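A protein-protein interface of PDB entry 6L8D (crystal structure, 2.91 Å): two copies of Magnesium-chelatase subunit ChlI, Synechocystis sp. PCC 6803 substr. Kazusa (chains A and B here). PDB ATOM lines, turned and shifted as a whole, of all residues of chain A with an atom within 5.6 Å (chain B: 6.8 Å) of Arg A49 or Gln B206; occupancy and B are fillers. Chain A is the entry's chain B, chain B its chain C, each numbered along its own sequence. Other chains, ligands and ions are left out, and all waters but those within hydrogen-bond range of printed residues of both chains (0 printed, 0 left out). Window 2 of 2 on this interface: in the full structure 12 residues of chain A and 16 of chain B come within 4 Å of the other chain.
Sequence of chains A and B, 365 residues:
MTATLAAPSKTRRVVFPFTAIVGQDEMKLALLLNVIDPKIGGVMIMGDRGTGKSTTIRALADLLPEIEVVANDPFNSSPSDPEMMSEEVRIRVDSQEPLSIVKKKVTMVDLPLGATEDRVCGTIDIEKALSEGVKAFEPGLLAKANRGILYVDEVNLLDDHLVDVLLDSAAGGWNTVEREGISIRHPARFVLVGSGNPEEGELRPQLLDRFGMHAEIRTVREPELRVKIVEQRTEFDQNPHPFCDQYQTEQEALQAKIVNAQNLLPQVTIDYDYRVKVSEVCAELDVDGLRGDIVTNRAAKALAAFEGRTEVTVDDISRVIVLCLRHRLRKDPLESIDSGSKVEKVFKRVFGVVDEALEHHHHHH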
ATOM      1  N   GLY A  47      20.297  -3.660  13.414  1.00  0.00           N
ATOM      2  CA  GLY A  47      19.640  -4.939  13.583  1.00  0.00           C
ATOM      3  C   GLY A  47      18.134  -4.877  13.693  1.00  0.00           C
ATOM      4  O   GLY A  47      17.493  -3.970  13.150  1.00  0.00           O
ATOM      5  N   ASP A  48      17.561  -5.856  14.388  1.00  0.00           N
ATOM      6  CA  ASP A  48      16.124  -5.896  14.591  1.00  0.00           C
ATOM      7  C   ASP A  48      15.654  -4.633  15.308  1.00  0.00           C
ATOM      8  O   ASP A  48      16.424  -3.929  15.967  1.00  0.00           O
ATOM      9  CB  ASP A  48      15.730  -7.146  15.383  1.00  0.00           C
ATOM     10  CG  ASP A  48      15.894  -8.426  14.573  1.00  0.00           C
ATOM     11  OD1 ASP A  48      16.115  -8.331  13.344  1.00  0.00           O
ATOM     12  OD2 ASP A  48      15.805  -9.525  15.162  1.00  0.00           O
ATOM     13  N   ARG A  49      14.388  -4.380  15.161  1.00  0.00           N
ATOM     14  CA  ARG A  49      13.799  -3.227  15.723  1.00  0.00           C
ATOM     15  C   ARG A  49      12.530  -3.677  16.346  1.00  0.00           C
ATOM     16  O   ARG A  49      11.573  -3.834  15.664  1.00  0.00           O
ATOM     17  CB  ARG A  49      13.479  -2.217  14.616  1.00  0.00           C
ATOM     18  CG  ARG A  49      13.903  -2.579  13.200  1.00  0.00           C
ATOM     19  CD  ARG A  49      12.866  -2.184  12.172  1.00  0.00           C
ATOM     20  NE  ARG A  49      11.518  -2.182  12.720  1.00  0.00           N
ATOM     21  CZ  ARG A  49      10.473  -2.744  12.145  1.00  0.00           C
ATOM     22  NH1 ARG A  49      10.613  -3.346  10.995  1.00  0.00           N
ATOM     23  NH2 ARG A  49       9.299  -2.699  12.732  1.00  0.00           N
ATOM     24  N   LYS A  53      15.756  -0.112  21.843  1.00  0.00           N
ATOM     25  CA  LYS A  53      17.021   0.525  21.496  1.00  0.00           C
ATOM     26  C   LYS A  53      17.122   1.919  22.105  1.00  0.00           C
ATOM     27  O   LYS A  53      18.129   2.265  22.724  1.00  0.00           O
ATOM     28  CB  LYS A  53      17.181   0.603  19.976  1.00  0.00           C
ATOM     29  CG  LYS A  53      18.479   0.002  19.458  1.00  0.00           C
ATOM     30  CD  LYS A  53      18.687   0.323  17.987  1.00  0.00           C
ATOM     31  CE  LYS A  53      17.423   0.065  17.181  1.00  0.00           C
ATOM     32  NZ  LYS A  53      17.727  -0.510  15.842  1.00  0.00           N
ATOM     33  N   ASN A 197      18.864   2.331   9.401  1.00  0.00           N
ATOM     34  CA  ASN A 197      17.869   1.493   8.770  1.00  0.00           C
ATOM     35  C   ASN A 197      18.448   0.794   7.553  1.00  0.00           C
ATOM     36  O   ASN A 197      19.005   1.455   6.664  1.00  0.00           O
ATOM     37  CB  ASN A 197      16.662   2.336   8.355  1.00  0.00           C
ATOM     38  CG  ASN A 197      15.535   1.501   7.799  1.00  0.00           C
ATOM     39  OD1 ASN A 197      15.522   0.280   7.936  1.00  0.00           O
ATOM     40  ND2 ASN A 197      14.578   2.159   7.164  1.00  0.00           N
ATOM     41  N   PRO A 198      18.330  -0.529   7.477  1.00  0.00           N
ATOM     42  CA  PRO A 198      18.701  -1.236   6.247  1.00  0.00           C
ATOM     43  C   PRO A 198      17.696  -0.957   5.137  1.00  0.00           C
ATOM     44  O   PRO A 198      16.540  -0.608   5.387  1.00  0.00           O
ATOM     45  CB  PRO A 198      18.699  -2.716   6.659  1.00  0.00           C
ATOM     46  CG  PRO A 198      18.689  -2.719   8.162  1.00  0.00           C
ATOM     47  CD  PRO A 198      18.024  -1.450   8.584  1.00  0.00           C
ATOM     48  N   GLU A 200      17.117   1.463   3.488  1.00  0.00           N
ATOM     49  CA  GLU A 200      16.990   2.908   3.337  1.00  0.00           C
ATOM     50  C   GLU A 200      18.344   3.591   3.298  1.00  0.00           C
ATOM     51  O   GLU A 200      18.434   4.803   3.556  1.00  0.00           O
ATOM     52  CB  GLU A 200      16.113   3.533   4.425  1.00  0.00           C
ATOM     53  CG  GLU A 200      14.624   3.437   4.116  1.00  0.00           C
ATOM     54  CD  GLU A 200      13.763   4.163   5.127  1.00  0.00           C
ATOM     55  OE1 GLU A 200      14.291   4.542   6.194  1.00  0.00           O
ATOM     56  OE2 GLU A 200      12.567   4.381   4.833  1.00  0.00           O
ATOM     57  N   THR A 219      16.721 -10.405  18.075  1.00  0.00           N
ATOM     58  CA  THR A 219      15.592 -10.580  18.976  1.00  0.00           C
ATOM     59  C   THR A 219      15.640 -11.952  19.638  1.00  0.00           C
ATOM     60  O   THR A 219      15.967 -12.960  19.002  1.00  0.00           O
ATOM     61  CB  THR A 219      14.279 -10.375  18.223  1.00  0.00           C
ATOM     62  OG1 THR A 219      14.388 -10.933  16.908  1.00  0.00           O
ATOM     63  CG2 THR A 219      13.995  -8.890  18.102  1.00  0.00           C
ATOM     64  N   LEU B 167       0.184   5.573  12.849  1.00  0.00           N
ATOM     65  CA  LEU B 167       0.537   4.388  13.621  1.00  0.00           C
ATOM     66  C   LEU B 167       0.965   4.750  15.035  1.00  0.00           C
ATOM     67  O   LEU B 167       0.787   3.949  15.962  1.00  0.00           O
ATOM     68  CB  LEU B 167       1.645   3.618  12.902  1.00  0.00           C
ATOM     69  CG  LEU B 167       1.267   2.976  11.568  1.00  0.00           C
ATOM     70  CD1 LEU B 167       2.511   2.616  10.770  1.00  0.00           C
ATOM     71  CD2 LEU B 167       0.419   1.736  11.819  1.00  0.00           C
ATOM     72  N   LEU B 203       3.256  -1.426   0.697  1.00  0.00           N
ATOM     73  CA  LEU B 203       3.773  -0.575   1.763  1.00  0.00           C
ATOM     74  C   LEU B 203       5.173  -1.008   2.185  1.00  0.00           C
ATOM     75  O   LEU B 203       5.598  -2.129   1.903  1.00  0.00           O
ATOM     76  CB  LEU B 203       2.830  -0.595   2.968  1.00  0.00           C
ATOM     77  N   ARG B 204       5.885  -0.112   2.860  1.00  0.00           N
ATOM     78  CA  ARG B 204       7.238  -0.400   3.322  1.00  0.00           C
ATOM     79  C   ARG B 204       7.263  -1.626   4.229  1.00  0.00           C
ATOM     80  O   ARG B 204       6.490  -1.710   5.188  1.00  0.00           O
ATOM     81  CB  ARG B 204       7.822   0.810   4.055  1.00  0.00           C
ATOM     82  N   PRO B 205       8.193  -2.604   3.896  1.00  0.00           N
ATOM     83  CA  PRO B 205       8.186  -3.770   4.796  1.00  0.00           C
ATOM     84  C   PRO B 205       8.344  -3.363   6.258  1.00  0.00           C
ATOM     85  O   PRO B 205       8.062  -4.159   7.153  1.00  0.00           O
ATOM     86  CB  PRO B 205       9.403  -4.583   4.346  1.00  0.00           C
ATOM     87  CG  PRO B 205       9.493  -4.322   2.893  1.00  0.00           C
ATOM     88  CD  PRO B 205       9.260  -2.847   2.822  1.00  0.00           C
ATOM     89  N   GLN B 206       8.791  -2.133   6.489  1.00  0.00           N
ATOM     90  CA  GLN B 206       8.982  -1.630   7.843  1.00  0.00           C
ATOM     91  C   GLN B 206       7.734  -0.950   8.397  1.00  0.00           C
ATOM     92  O   GLN B 206       7.584  -0.865   9.622  1.00  0.00           O
ATOM     93  CB  GLN B 206      10.203  -0.704   7.882  1.00  0.00           C
ATOM     94  CG  GLN B 206      10.654  -0.319   9.285  1.00  0.00           C
ATOM     95  CD  GLN B 206      11.816   0.653   9.272  1.00  0.00           C
ATOM     96  OE1 GLN B 206      12.358   0.969   8.213  1.00  0.00           O
ATOM     97  NE2 GLN B 206      12.236   1.094  10.455  1.00  0.00           N
ATOM     98  N   LEU B 207       6.837  -0.469   7.528  1.00  0.00           N
ATOM     99  CA  LEU B 207       5.609   0.192   7.960  1.00  0.00           C
ATOM    100  C   LEU B 207       4.395  -0.726   7.927  1.00  0.00           C
ATOM    101  O   LEU B 207       3.319  -0.319   8.372  1.00  0.00           O
ATOM    102  CB  LEU B 207       5.323   1.437   7.107  1.00  0.00           C
ATOM    103  CG  LEU B 207       5.627   2.800   7.746  1.00  0.00           C
ATOM    104  CD1 LEU B 207       6.979   2.815   8.455  1.00  0.00           C
ATOM    105  CD2 LEU B 207       5.534   3.911   6.705  1.00  0.00           C
ATOM    106  N   LEU B 208       4.545  -1.951   7.437  1.00  0.00           N
ATOM    107  CA  LEU B 208       3.465  -2.924   7.482  1.00  0.00           C
ATOM    108  C   LEU B 208       3.537  -3.753   8.753  1.00  0.00           C
ATOM    109  O   LEU B 208       2.498  -4.152   9.290  1.00  0.00           O
ATOM    110  CB  LEU B 208       3.518  -3.840   6.258  1.00  0.00           C
ATOM    111  CG  LEU B 208       2.687  -5.120   6.335  1.00  0.00           C
ATOM    112  CD1 LEU B 208       1.204  -4.810   6.196  1.00  0.00           C
ATOM    113  CD2 LEU B 208       3.140  -6.128   5.292  1.00  0.00           C
ATOM    114  N   ASP B 209       4.751  -3.997   9.255  1.00  0.00           N
ATOM    115  CA  ASP B 209       4.931  -4.681  10.528  1.00  0.00           C
ATOM    116  C   ASP B 209       4.267  -3.925  11.668  1.00  0.00           C
ATOM    117  O   ASP B 209       3.947  -4.528  12.698  1.00  0.00           O
ATOM    118  CB  ASP B 209       6.423  -4.835  10.839  1.00  0.00           C
ATOM    119  CG  ASP B 209       7.167  -5.663   9.795  1.00  0.00           C
ATOM    120  OD1 ASP B 209       6.527  -6.120   8.821  1.00  0.00           O
ATOM    121  OD2 ASP B 209       8.400  -5.848   9.945  1.00  0.00           O
ATOM    122  N   ARG B 210       4.049  -2.618  11.505  1.00  0.00           N
ATOM    123  CA  ARG B 210       3.475  -1.794  12.560  1.00  0.00           C
ATOM    124  C   ARG B 210       1.958  -1.901  12.626  1.00  0.00           C
ATOM    125  O   ARG B 210       1.360  -1.419  13.596  1.00  0.00           O
ATOM    126  CB  ARG B 210       3.888  -0.337  12.335  1.00  0.00           C
ATOM    127  CG  ARG B 210       5.400  -0.128  12.332  1.00  0.00           C
ATOM    128  CD  ARG B 210       5.799   1.339  12.180  1.00  0.00           C
ATOM    129  NE  ARG B 210       5.106   2.227  13.106  1.00  0.00           N
ATOM    130  CZ  ARG B 210       5.381   2.324  14.400  1.00  0.00           C
ATOM    131  NH1 ARG B 210       6.346   1.584  14.932  1.00  0.00           N
ATOM    132  NH2 ARG B 210       4.690   3.163  15.164  1.00  0.00           N
ATOM    133  N   PHE B 211       1.331  -2.531  11.634  1.00  0.00           N
ATOM    134  CA  PHE B 211      -0.092  -2.826  11.675  1.00  0.00           C
ATOM    135  C   PHE B 211      -0.362  -4.064  12.518  1.00  0.00           C
ATOM    136  O   PHE B 211       0.350  -5.068  12.416  1.00  0.00           O
ATOM    137  CB  PHE B 211      -0.631  -3.022  10.263  1.00  0.00           C
ATOM    138  CG  PHE B 211      -1.148  -1.767   9.645  1.00  0.00           C
ATOM    139  CD1 PHE B 211      -0.359  -1.034   8.779  1.00  0.00           C
ATOM    140  CD2 PHE B 211      -2.416  -1.306   9.947  1.00  0.00           C
ATOM    141  CE1 PHE B 211      -0.829   0.130   8.209  1.00  0.00           C
ATOM    142  CE2 PHE B 211      -2.893  -0.144   9.386  1.00  0.00           C
ATOM    143  CZ  PHE B 211      -2.098   0.577   8.514  1.00  0.00           C
ATOM    144  N   ASP B 288      10.230 -10.048  13.658  1.00  0.00           N
ATOM    145  CA  ASP B 288      11.040  -8.869  13.973  1.00  0.00           C
ATOM    146  C   ASP B 288      10.514  -8.240  15.259  1.00  0.00           C
ATOM    147  O   ASP B 288       9.606  -7.409  15.244  1.00  0.00           O
ATOM    148  CB  ASP B 288      10.998  -7.882  12.813  1.00  0.00           C
ATOM    149  CG  ASP B 288      12.093  -6.829  12.886  1.00  0.00           C
ATOM    150  OD1 ASP B 288      12.427  -6.361  13.993  1.00  0.00           O
ATOM    151  OD2 ASP B 288      12.613  -6.458  11.813  1.00  0.00           O
ATOM    152  N   GLY B 289      11.101  -8.609  16.385  1.00  0.00           N
ATOM    153  CA  GLY B 289      10.711  -8.013  17.642  1.00  0.00           C
ATOM    154  C   GLY B 289       9.718  -8.878  18.387  1.00  0.00           C
ATOM    155  O   GLY B 289       9.503 -10.051  18.074  1.00  0.00           O
ATOM    156  N   LEU B 290       9.101  -8.274  19.400  1.00  0.00           N
ATOM    157  CA  LEU B 290       8.111  -8.958  20.220  1.00  0.00           C
ATOM    158  C   LEU B 290       6.694  -8.475  19.938  1.00  0.00           C
ATOM    159  O   LEU B 290       5.757  -8.874  20.638  1.00  0.00           O
ATOM    160  CB  LEU B 290       8.443  -8.781  21.700  1.00  0.00           C
ATOM    161  CG  LEU B 290       9.764  -9.391  22.162  1.00  0.00           C
ATOM    162  CD1 LEU B 290       9.894  -9.261  23.663  1.00  0.00           C
ATOM    163  CD2 LEU B 290       9.883 -10.838  21.726  1.00  0.00           C
ATOM    164  N   ARG B 330       9.562 -13.489   8.111  1.00  0.00           N
ATOM    165  CA  ARG B 330      10.842 -13.328   7.434  1.00  0.00           C
ATOM    166  C   ARG B 330      11.190 -14.671   6.791  1.00  0.00           C
ATOM    167  O   ARG B 330      12.050 -15.412   7.282  1.00  0.00           O
ATOM    168  CB  ARG B 330      11.925 -12.858   8.413  1.00  0.00           C
ATOM    169  CG  ARG B 330      11.745 -11.422   8.888  1.00  0.00           C
ATOM    170  CD  ARG B 330      13.068 -10.679   8.884  1.00  0.00           C
ATOM    171  NE  ARG B 330      13.240  -9.804  10.041  1.00  0.00           N
ATOM    172  CZ  ARG B 330      13.670 -10.218  11.228  1.00  0.00           C
ATOM    173  NH1 ARG B 330      13.958 -11.496  11.420  1.00  0.00           N
ATOM    174  NH2 ARG B 330      13.814  -9.355  12.225  1.00  0.00           N
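The side-chain carboxylate (OD1) of Asp A48 is in salt-bridge range of the guanidinium group (NH2) of Arg B330 (2.8 Å).
The guanidinium group (NH1) of Arg A49 lies within salt-bridge range of the side-chain carboxylate (OD2) of Asp B209.
NH1 of Arg A49 is in salt-bridge range of OD2 of Asp B288 (3.8 Å).
The side-chain amide nitrogen of Asn A197 sits at hydrogen-bond distance from the side-chain amide oxygen of Gln B206 (2.7 Å).
No position is printed for both chains.
Of the 7 pairs that touch across the chains among the printed residues, none has its exchanged pair printed and touching as well.
OD2 of Asp A48 is in hydrogen-bond range of OG1 of Thr A219, at 2.7 Å.
ND2 of Asn A197 is in hydrogen-bond range of OE1 of Glu A200 (2.6 Å).
The side-chain carboxylate of Asp B288 lies within salt-bridge range of the guanidinium group of Arg B330 (3.2 Å).
Of the 8 printed residues of chain A, 4 touch a printed residue of chain B.
Along chain A the printed residues that touch a printed residue of chain B span positions 48 to 219.
Among the printed residues, 7 pairs touch across the chains.
Among the printed residues, pairs that only touch across the chains: Thr A219 with Gly B289 (3.4 Å), Arg A49 with Gln B206 (3.5 Å) and Asp A48 with Asp B288 (3.7 Å).
Printed residues of chain B within 4 Å of Asp A48: Asp B288 (3.7 Å) and Arg B330 (2.8 Å).
Arg A49 touches three residues of chain B.
Printed residues of chain B within 4 Å of Asn A197: Gln B206.
Of chain A, only Arg A49 (3.5 Å) and Asn A197 (2.7 Å) come within 4 Å of Gln B206.
Of the printed residues of chain A, Asp B209 touches Arg A49.
Of the printed residues of chain A, Gly B289 touches Thr A219.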
